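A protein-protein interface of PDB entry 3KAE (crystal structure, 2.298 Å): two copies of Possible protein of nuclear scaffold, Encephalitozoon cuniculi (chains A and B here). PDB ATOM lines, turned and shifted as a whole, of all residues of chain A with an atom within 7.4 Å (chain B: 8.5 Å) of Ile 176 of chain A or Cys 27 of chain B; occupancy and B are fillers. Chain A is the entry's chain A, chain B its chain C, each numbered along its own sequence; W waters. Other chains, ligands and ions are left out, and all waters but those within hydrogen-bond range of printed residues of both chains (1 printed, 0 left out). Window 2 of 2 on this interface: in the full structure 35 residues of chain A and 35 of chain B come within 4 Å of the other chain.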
ATOM      1  N   PHE A 145      11.572  11.221  21.771  1.00  0.00           N
ATOM      2  CA  PHE A 145      12.676  11.814  21.030  1.00  0.00           C
ATOM      3  C   PHE A 145      13.986  11.067  21.305  1.00  0.00           C
ATOM      4  O   PHE A 145      14.406  10.961  22.452  1.00  0.00           O
ATOM      5  CB  PHE A 145      12.875  13.276  21.426  1.00  0.00           C
ATOM      6  CG  PHE A 145      14.108  13.913  20.806  1.00  0.00           C
ATOM      7  CD1 PHE A 145      15.391  13.630  21.290  1.00  0.00           C
ATOM      8  CD2 PHE A 145      13.983  14.785  19.731  1.00  0.00           C
ATOM      9  CE1 PHE A 145      16.519  14.205  20.710  1.00  0.00           C
ATOM     10  CE2 PHE A 145      15.104  15.374  19.154  1.00  0.00           C
ATOM     11  CZ  PHE A 145      16.378  15.081  19.642  1.00  0.00           C
ATOM     12  N   GLY A 175       8.622  20.160  24.383  1.00  0.00           N
ATOM     13  CA  GLY A 175      10.042  20.189  24.684  1.00  0.00           C
ATOM     14  C   GLY A 175      10.821  21.086  23.737  1.00  0.00           C
ATOM     15  O   GLY A 175      10.356  21.414  22.634  1.00  0.00           O
ATOM     16  N   ILE A 176      12.009  21.497  24.169  1.00  0.00           N
ATOM     17  CA  ILE A 176      12.881  22.286  23.312  1.00  0.00           C
ATOM     18  C   ILE A 176      13.311  21.435  22.128  1.00  0.00           C
ATOM     19  O   ILE A 176      13.495  21.944  21.019  1.00  0.00           O
ATOM     20  CB  ILE A 176      14.113  22.831  24.077  1.00  0.00           C
ATOM     21  CG1 ILE A 176      15.202  23.295  23.093  1.00  0.00           C
ATOM     22  CG2 ILE A 176      14.639  21.778  25.063  1.00  0.00           C
ATOM     23  CD1 ILE A 176      16.259  24.210  23.702  1.00  0.00           C
ATOM     24  N   GLU A 177      13.457  20.132  22.355  1.00  0.00           N
ATOM     25  CA  GLU A 177      13.843  19.252  21.266  1.00  0.00           C
ATOM     26  C   GLU A 177      12.675  19.094  20.281  1.00  0.00           C
ATOM     27  O   GLU A 177      12.862  19.061  19.060  1.00  0.00           O
ATOM     28  CB  GLU A 177      14.382  17.907  21.782  1.00  0.00           C
ATOM     29  CG  GLU A 177      13.351  16.945  22.359  1.00  0.00           C
ATOM     30  CD  GLU A 177      12.970  17.254  23.798  1.00  0.00           C
ATOM     31  OE1 GLU A 177      13.079  18.436  24.210  1.00  0.00           O
ATOM     32  OE2 GLU A 177      12.552  16.311  24.511  1.00  0.00           O
ATOM     33  N   GLU A 178      11.459  19.045  20.806  1.00  0.00           N
ATOM     34  CA  GLU A 178      10.292  18.849  19.951  1.00  0.00           C
ATOM     35  C   GLU A 178      10.021  20.108  19.115  1.00  0.00           C
ATOM     36  O   GLU A 178       9.504  20.049  17.992  1.00  0.00           O
ATOM     37  CB  GLU A 178       9.065  18.436  20.778  1.00  0.00           C
ATOM     38  CG  GLU A 178       9.319  17.294  21.788  1.00  0.00           C
ATOM     39  CD  GLU A 178       9.675  15.942  21.140  1.00  0.00           C
ATOM     40  OE1 GLU A 178       9.547  15.806  19.901  1.00  0.00           O
ATOM     41  OE2 GLU A 178      10.074  15.009  21.880  1.00  0.00           O
ATOM     42  N   GLU A 179      10.386  21.254  19.670  1.00  0.00           N
ATOM     43  CA  GLU A 179      10.398  22.486  18.907  1.00  0.00           C
ATOM     44  C   GLU A 179      11.479  22.489  17.817  1.00  0.00           C
ATOM     45  O   GLU A 179      11.270  23.053  16.733  1.00  0.00           O
ATOM     46  CB  GLU A 179      10.624  23.658  19.857  1.00  0.00           C
ATOM     47  CG  GLU A 179      10.960  24.962  19.172  1.00  0.00           C
ATOM     48  CD  GLU A 179      11.081  26.104  20.160  1.00  0.00           C
ATOM     49  OE1 GLU A 179      10.855  25.864  21.364  1.00  0.00           O
ATOM     50  OE2 GLU A 179      11.394  27.238  19.738  1.00  0.00           O
ATOM     51  N   TYR A 180      12.632  21.880  18.116  1.00  0.00           N
ATOM     52  CA  TYR A 180      13.720  21.767  17.151  1.00  0.00           C
ATOM     53  C   TYR A 180      13.271  20.938  15.957  1.00  0.00           C
ATOM     54  O   TYR A 180      13.622  21.226  14.814  1.00  0.00           O
ATOM     55  CB  TYR A 180      14.961  21.109  17.802  1.00  0.00           C
ATOM     56  CG  TYR A 180      15.919  20.471  16.814  1.00  0.00           C
ATOM     57  CD1 TYR A 180      15.813  19.123  16.491  1.00  0.00           C
ATOM     58  CD2 TYR A 180      16.926  21.217  16.199  1.00  0.00           C
ATOM     59  CE1 TYR A 180      16.697  18.530  15.592  1.00  0.00           C
ATOM     60  CE2 TYR A 180      17.808  20.636  15.281  1.00  0.00           C
ATOM     61  CZ  TYR A 180      17.684  19.295  14.985  1.00  0.00           C
ATOM     62  OH  TYR A 180      18.546  18.681  14.091  1.00  0.00           O
ATOM     63  N   VAL A 181      12.518  19.882  16.235  1.00  0.00           N
ATOM     64  CA  VAL A 181      11.981  19.035  15.184  1.00  0.00           C
ATOM     65  C   VAL A 181      10.939  19.821  14.369  1.00  0.00           C
ATOM     66  O   VAL A 181      10.928  19.779  13.138  1.00  0.00           O
ATOM     67  CB  VAL A 181      11.328  17.783  15.770  1.00  0.00           C
ATOM     68  CG1 VAL A 181      10.838  16.880  14.653  1.00  0.00           C
ATOM     69  CG2 VAL A 181      12.308  17.055  16.692  1.00  0.00           C
ATOM     70  N   SER A 182      10.067  20.542  15.061  1.00  0.00           N
ATOM     71  CA  SER A 182       9.041  21.337  14.360  1.00  0.00           C
ATOM     72  C   SER A 182       9.699  22.312  13.398  1.00  0.00           C
ATOM     73  O   SER A 182       9.330  22.390  12.230  1.00  0.00           O
ATOM     74  CB  SER A 182       8.153  22.101  15.346  1.00  0.00           C
ATOM     75  OG  SER A 182       7.694  21.243  16.382  1.00  0.00           O
ATOM     76  N   ASP A 183      10.695  23.041  13.893  1.00  0.00           N
ATOM     77  CA  ASP A 183      11.397  24.037  13.083  1.00  0.00           C
ATOM     78  C   ASP A 183      12.062  23.390  11.881  1.00  0.00           C
ATOM     79  O   ASP A 183      12.043  23.959  10.782  1.00  0.00           O
ATOM     80  CB  ASP A 183      12.457  24.749  13.922  1.00  0.00           C
ATOM     81  CG  ASP A 183      11.850  25.614  15.013  1.00  0.00           C
ATOM     82  OD1 ASP A 183      10.601  25.715  15.068  1.00  0.00           O
ATOM     83  OD2 ASP A 183      12.621  26.200  15.809  1.00  0.00           O
ATOM     84  N   TYR A 199      18.417  30.099  14.876  1.00  0.00           N
ATOM     85  CA  TYR A 199      19.346  29.058  15.334  1.00  0.00           C
ATOM     86  C   TYR A 199      20.814  29.435  15.153  1.00  0.00           C
ATOM     87  O   TYR A 199      21.711  28.752  15.660  1.00  0.00           O
ATOM     88  CB  TYR A 199      19.051  27.729  14.638  1.00  0.00           C
ATOM     89  CG  TYR A 199      17.839  27.019  15.211  1.00  0.00           C
ATOM     90  CD1 TYR A 199      17.978  26.101  16.236  1.00  0.00           C
ATOM     91  CD2 TYR A 199      16.549  27.281  14.731  1.00  0.00           C
ATOM     92  CE1 TYR A 199      16.881  25.451  16.772  1.00  0.00           C
ATOM     93  CE2 TYR A 199      15.438  26.634  15.264  1.00  0.00           C
ATOM     94  CZ  TYR A 199      15.611  25.726  16.286  1.00  0.00           C
ATOM     95  OH  TYR A 199      14.530  25.074  16.829  1.00  0.00           O
ATOM     96  N   HIS A 202      22.760  30.095  18.383  1.00  0.00           N
ATOM     97  CA  HIS A 202      23.095  28.974  19.265  1.00  0.00           C
ATOM     98  C   HIS A 202      24.107  28.007  18.640  1.00  0.00           C
ATOM     99  O   HIS A 202      23.870  26.805  18.540  1.00  0.00           O
ATOM    100  CB  HIS A 202      21.831  28.240  19.700  1.00  0.00           C
ATOM    101  CG  HIS A 202      20.782  29.142  20.261  1.00  0.00           C
ATOM    102  ND1 HIS A 202      20.802  29.589  21.566  1.00  0.00           N
ATOM    103  CD2 HIS A 202      19.680  29.691  19.694  1.00  0.00           C
ATOM    104  CE1 HIS A 202      19.757  30.373  21.775  1.00  0.00           C
ATOM    105  NE2 HIS A 202      19.060  30.451  20.657  1.00  0.00           N
ATOM    106  N   GLY A 205      25.967  24.679  19.833  1.00  0.00           N
ATOM    107  CA  GLY A 205      24.756  24.333  20.555  1.00  0.00           C
ATOM    108  C   GLY A 205      23.754  23.669  19.635  1.00  0.00           C
ATOM    109  O   GLY A 205      24.135  23.071  18.624  1.00  0.00           O
ATOM    110  N   ILE A 206      22.472  23.794  19.973  1.00  0.00           N
ATOM    111  CA  ILE A 206      21.403  23.271  19.126  1.00  0.00           C
ATOM    112  C   ILE A 206      21.474  23.839  17.706  1.00  0.00           C
ATOM    113  O   ILE A 206      21.092  23.186  16.735  1.00  0.00           O
ATOM    114  CB  ILE A 206      20.018  23.550  19.737  1.00  0.00           C
ATOM    115  CG1 ILE A 206      18.938  22.759  19.007  1.00  0.00           C
ATOM    116  CG2 ILE A 206      19.688  25.025  19.702  1.00  0.00           C
ATOM    117  CD1 ILE A 206      17.587  22.822  19.693  1.00  0.00           C
ATOM    118  N   TYR A 209      23.422  21.774  14.991  1.00  0.00           N
ATOM    119  CA  TYR A 209      22.622  20.767  14.292  1.00  0.00           C
ATOM    120  C   TYR A 209      21.718  21.401  13.237  1.00  0.00           C
ATOM    121  O   TYR A 209      21.794  21.058  12.053  1.00  0.00           O
ATOM    122  CB  TYR A 209      21.784  19.952  15.283  1.00  0.00           C
ATOM    123  CG  TYR A 209      22.603  19.228  16.306  1.00  0.00           C
ATOM    124  CD1 TYR A 209      23.078  17.942  16.058  1.00  0.00           C
ATOM    125  CD2 TYR A 209      22.916  19.823  17.522  1.00  0.00           C
ATOM    126  CE1 TYR A 209      23.829  17.270  16.981  1.00  0.00           C
ATOM    127  CE2 TYR A 209      23.674  19.154  18.462  1.00  0.00           C
ATOM    128  CZ  TYR A 209      24.129  17.874  18.189  1.00  0.00           C
ATOM    129  OH  TYR A 209      24.893  17.197  19.126  1.00  0.00           O
ATOM    130  N   LEU B   5      14.683  17.214  30.991  1.00  0.00           N
ATOM    131  CA  LEU B   5      15.760  16.801  30.095  1.00  0.00           C
ATOM    132  C   LEU B   5      16.811  15.938  30.829  1.00  0.00           C
ATOM    133  O   LEU B   5      17.461  15.090  30.221  1.00  0.00           O
ATOM    134  CB  LEU B   5      16.420  18.014  29.426  1.00  0.00           C
ATOM    135  CG  LEU B   5      15.685  18.648  28.229  1.00  0.00           C
ATOM    136  CD1 LEU B   5      16.377  19.914  27.671  1.00  0.00           C
ATOM    137  CD2 LEU B   5      15.489  17.621  27.118  1.00  0.00           C
ATOM    138  N   ILE B   9      18.489  12.373  29.774  1.00  0.00           N
ATOM    139  CA  ILE B   9      19.905  12.280  29.474  1.00  0.00           C
ATOM    140  C   ILE B   9      20.490  11.062  30.202  1.00  0.00           C
ATOM    141  O   ILE B   9      21.199  10.256  29.601  1.00  0.00           O
ATOM    142  CB  ILE B   9      20.655  13.576  29.849  1.00  0.00           C
ATOM    143  CG1 ILE B   9      20.285  14.696  28.889  1.00  0.00           C
ATOM    144  CG2 ILE B   9      22.186  13.356  29.820  1.00  0.00           C
ATOM    145  CD1 ILE B   9      20.645  16.115  29.367  1.00  0.00           C
ATOM    146  N   THR B  20      22.072  11.100  21.480  1.00  0.00           N
ATOM    147  CA  THR B  20      20.913  11.716  22.107  1.00  0.00           C
ATOM    148  C   THR B  20      21.309  12.532  23.329  1.00  0.00           C
ATOM    149  O   THR B  20      20.829  13.639  23.525  1.00  0.00           O
ATOM    150  CB  THR B  20      19.881  10.663  22.502  1.00  0.00           C
ATOM    151  OG1 THR B  20      19.446   9.991  21.322  1.00  0.00           O
ATOM    152  CG2 THR B  20      18.712  11.284  23.198  1.00  0.00           C
ATOM    153  N   ALA B  21      22.194  11.989  24.150  1.00  0.00           N
ATOM    154  CA  ALA B  21      22.601  12.657  25.382  1.00  0.00           C
ATOM    155  C   ALA B  21      23.360  13.938  25.098  1.00  0.00           C
ATOM    156  O   ALA B  21      23.216  14.923  25.808  1.00  0.00           O
ATOM    157  CB  ALA B  21      23.466  11.701  26.241  1.00  0.00           C
ATOM    158  N   ILE B  22      24.219  13.893  24.090  1.00  0.00           N
ATOM    159  CA  ILE B  22      24.955  15.059  23.658  1.00  0.00           C
ATOM    160  C   ILE B  22      23.946  16.130  23.132  1.00  0.00           C
ATOM    161  O   ILE B  22      24.002  17.307  23.506  1.00  0.00           O
ATOM    162  CB  ILE B  22      26.000  14.658  22.601  1.00  0.00           C
ATOM    163  CG1 ILE B  22      27.096  13.784  23.256  1.00  0.00           C
ATOM    164  CG2 ILE B  22      26.620  15.888  21.964  1.00  0.00           C
ATOM    165  CD1 ILE B  22      28.030  13.091  22.276  1.00  0.00           C
ATOM    166  N   PHE B  23      22.999  15.713  22.299  1.00  0.00           N
ATOM    167  CA  PHE B  23      21.986  16.638  21.786  1.00  0.00           C
ATOM    168  C   PHE B  23      21.143  17.241  22.907  1.00  0.00           C
ATOM    169  O   PHE B  23      21.019  18.453  23.016  1.00  0.00           O
ATOM    170  CB  PHE B  23      21.069  15.954  20.777  1.00  0.00           C
ATOM    171  CG  PHE B  23      20.072  16.879  20.158  1.00  0.00           C
ATOM    172  CD1 PHE B  23      18.889  17.186  20.815  1.00  0.00           C
ATOM    173  CD2 PHE B  23      20.319  17.455  18.918  1.00  0.00           C
ATOM    174  CE1 PHE B  23      17.971  18.051  20.251  1.00  0.00           C
ATOM    175  CE2 PHE B  23      19.402  18.315  18.345  1.00  0.00           C
ATOM    176  CZ  PHE B  23      18.222  18.622  19.014  1.00  0.00           C
ATOM    177  N   LEU B  24      20.573  16.394  23.746  1.00  0.00           N
ATOM    178  CA  LEU B  24      19.774  16.878  24.867  1.00  0.00           C
ATOM    179  C   LEU B  24      20.596  17.744  25.807  1.00  0.00           C
ATOM    180  O   LEU B  24      20.065  18.623  26.480  1.00  0.00           O
ATOM    181  CB  LEU B  24      19.186  15.694  25.653  1.00  0.00           C
ATOM    182  CG  LEU B  24      18.124  14.849  24.966  1.00  0.00           C
ATOM    183  CD1 LEU B  24      17.642  13.764  25.910  1.00  0.00           C
ATOM    184  CD2 LEU B  24      16.949  15.751  24.517  1.00  0.00           C
ATOM    185  N   ALA B  25      21.894  17.481  25.867  1.00  0.00           N
ATOM    186  CA  ALA B  25      22.764  18.249  26.740  1.00  0.00           C
ATOM    187  C   ALA B  25      22.940  19.622  26.125  1.00  0.00           C
ATOM    188  O   ALA B  25      22.910  20.644  26.821  1.00  0.00           O
ATOM    189  CB  ALA B  25      24.116  17.540  26.918  1.00  0.00           C
ATOM    190  N   ALA B  26      23.110  19.637  24.806  1.00  0.00           N
ATOM    191  CA  ALA B  26      23.275  20.888  24.069  1.00  0.00           C
ATOM    192  C   ALA B  26      22.077  21.822  24.265  1.00  0.00           C
ATOM    193  O   ALA B  26      22.240  23.051  24.292  1.00  0.00           O
ATOM    194  CB  ALA B  26      23.519  20.609  22.577  1.00  0.00           C
ATOM    195  N   CYS B  27      20.883  21.239  24.415  1.00  0.00           N
ATOM    196  CA  CYS B  27      19.654  22.030  24.598  1.00  0.00           C
ATOM    197  C   CYS B  27      19.660  22.647  25.975  1.00  0.00           C
ATOM    198  O   CYS B  27      19.076  23.702  26.196  1.00  0.00           O
ATOM    199  CB  CYS B  27      18.389  21.167  24.469  1.00  0.00           C
ATOM    200  SG  CYS B  27      18.157  20.409  22.867  1.00  0.00           S
ATOM    201  N   LEU B  28      20.330  21.969  26.903  1.00  0.00           N
ATOM    202  CA  LEU B  28      20.269  22.319  28.316  1.00  0.00           C
ATOM    203  C   LEU B  28      21.252  23.421  28.711  1.00  0.00           C
ATOM    204  O   LEU B  28      21.010  24.155  29.670  1.00  0.00           O
ATOM    205  CB  LEU B  28      20.512  21.074  29.162  1.00  0.00           C
ATOM    206  CG  LEU B  28      19.885  21.108  30.548  1.00  0.00           C
ATOM    207  CD1 LEU B  28      18.405  21.385  30.447  1.00  0.00           C
ATOM    208  CD2 LEU B  28      20.135  19.795  31.247  1.00  0.00           C
ATOM    209  N   LEU B  29      22.356  23.532  27.978  1.00  0.00           N
ATOM    210  CA  LEU B  29      23.334  24.600  28.196  1.00  0.00           C
ATOM    211  C   LEU B  29      22.729  25.977  28.571  1.00  0.00           C
ATOM    212  O   LEU B  29      23.202  26.630  29.502  1.00  0.00           O
ATOM    213  CB  LEU B  29      24.225  24.755  26.959  1.00  0.00           C
ATOM    214  CG  LEU B  29      25.205  23.628  26.643  1.00  0.00           C
ATOM    215  CD1 LEU B  29      25.892  23.891  25.298  1.00  0.00           C
ATOM    216  CD2 LEU B  29      26.215  23.503  27.764  1.00  0.00           C
ATOM    217  N   PRO B  30      21.700  26.440  27.834  1.00  0.00           N
ATOM    218  CA  PRO B  30      21.097  27.758  28.123  1.00  0.00           C
ATOM    219  C   PRO B  30      20.380  27.820  29.476  1.00  0.00           C
ATOM    220  O   PRO B  30      20.848  28.511  30.384  1.00  0.00           O
ATOM    221  CB  PRO B  30      20.074  27.952  26.989  1.00  0.00           C
ATOM    222  CG  PRO B  30      20.490  26.990  25.917  1.00  0.00           C
ATOM    223  CD  PRO B  30      21.122  25.818  26.630  1.00  0.00           C
ATOM    224  N   CYS B  31      19.251  27.118  29.582  1.00  0.00           N
ATOM    225  CA  CYS B  31      18.504  26.984  30.833  1.00  0.00           C
ATOM    226  C   CYS B  31      19.423  26.892  32.054  1.00  0.00           C
ATOM    227  O   CYS B  31      19.503  27.830  32.853  1.00  0.00           O
ATOM    228  CB  CYS B  31      17.612  25.734  30.787  1.00  0.00           C
ATOM    229  SG  CYS B  31      16.487  25.639  29.365  1.00  0.00           S
ATOM    230  N   LYS B  32      20.117  25.760  32.192  1.00  0.00           N
ATOM    231  CA  LYS B  32      20.939  25.523  33.370  1.00  0.00           C
ATOM    232  C   LYS B  32      22.407  25.277  33.016  1.00  0.00           C
ATOM    233  O   LYS B  32      22.786  24.149  32.665  1.00  0.00           O
ATOM    234  CB  LYS B  32      20.369  24.357  34.182  1.00  0.00           C
ATOM    235  N   PRO B  33      23.233  26.338  33.096  1.00  0.00           N
ATOM    236  CA  PRO B  33      24.675  26.306  32.809  1.00  0.00           C
ATOM    237  C   PRO B  33      25.459  25.460  33.810  1.00  0.00           C
ATOM    238  O   PRO B  33      26.592  25.069  33.523  1.00  0.00           O
ATOM    239  CB  PRO B  33      25.100  27.769  32.939  1.00  0.00           C
ATOM    240  CG  PRO B  33      23.831  28.560  32.806  1.00  0.00           C
ATOM    241  CD  PRO B  33      22.761  27.701  33.391  1.00  0.00           C
ATOM    242  N   MET B  39      27.734  17.829  29.720  1.00  0.00           N
ATOM    243  CA  MET B  39      28.030  17.848  28.305  1.00  0.00           C
ATOM    244  C   MET B  39      29.432  17.288  28.073  1.00  0.00           C
ATOM    245  O   MET B  39      29.646  16.451  27.202  1.00  0.00           O
ATOM    246  CB  MET B  39      27.949  19.298  27.819  1.00  0.00           C
ATOM    247  CG  MET B  39      28.390  19.523  26.396  1.00  0.00           C
ATOM    248  SD  MET B  39      27.285  18.791  25.194  1.00  0.00           S
ATOM    249  CE  MET B  39      27.613  19.870  23.805  1.00  0.00           C
HETATM  250  O   HOH W   1      21.914  25.330  22.193  1.00  0.00           O
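CZ of Phe 145 of chain A touches CE1 of Phe 23 of chain B, 3.4 Å away. Ile 176 of chain A touches Leu 5 of chain B (CG2 to CD1, 3.6 Å). Cys 27 of chain B touches Ile 176 of chain A (CB to CD1, 3.8 Å). Leu 5 of chain B touches Glu 177 of chain A (CD2 to OE1, 3.9 Å). Phe 23 of chain B touches Glu 177 of chain A (CE1 to CB, 3.9 Å). CZ of Phe 23 of chain B touches CD1 of Tyr 180 of chain A, at 3.5 Å. OH of Tyr 209 of chain A touches CG2 of Ile 22 of chain B, at 3.6 Å. Tyr 209 of chain A touches Phe 23 of chain B (CD2 to CD2, 3.8 Å).
The backbone carbonyl oxygen (O) of Phe 23 of chain B lies within hydrogen-bond range of the side-chain sulfur (SG) of Cys 27 of chain B (3.5 Å).
Of the 15 printed residues of chain A, 5 touch a printed residue of chain B. Hydrophobic or aromatic side chains of chain A that line the printed part of chain B: Phe 145, Ile 176, Tyr 180 and Tyr 209. Of the 17 printed residues of chain B, 4 touch a printed residue of chain A. Printed residues of chain B that touch a printed residue of chain A: Leu 5, Ile 22, Phe 23 and Cys 27. Hydrophobic or aromatic side chains of chain B within 4 Å of the printed part of chain A: Leu 5, Ile 22 and Phe 23.
No position is printed for both chains.
Water W1 lies within hydrogen-bond range of N of Ile 206 of chain A (2.8 Å) and O of Ala 26 of chain B (3.1 Å).
Cys 27 of chain B touches one residue of chain A. No residue of chain A comes within 4 Å of Ala 26 of chain B. Printed residues of chain A within 4 Å of Phe 23 of chain B: Phe 145, Glu 177, Tyr 180 and Tyr 209. Printed residues of chain B within 4 Å of Tyr 209 of chain A: Ile 22 (3.6 Å) and Phe 23 (3.8 Å). Printed residues of chain B within 4 Å of Glu 177 of chain A: Leu 5 and Phe 23. Of the printed residues of chain B, Phe 145 of chain A touches Phe 23 (3.4 Å). Glu 179 of chain A touches none of the printed residues of chain B. Ala 21 of chain B touches none of the printed residues of chain A. The nearest residue of chain A that does not touch Cys 27 of chain B is Ile 206 of chain A (4.03 Å). The nearest printed residue of chain A that does not touch Phe 23 of chain B is Ile 206 of chain A (4.2 Å).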
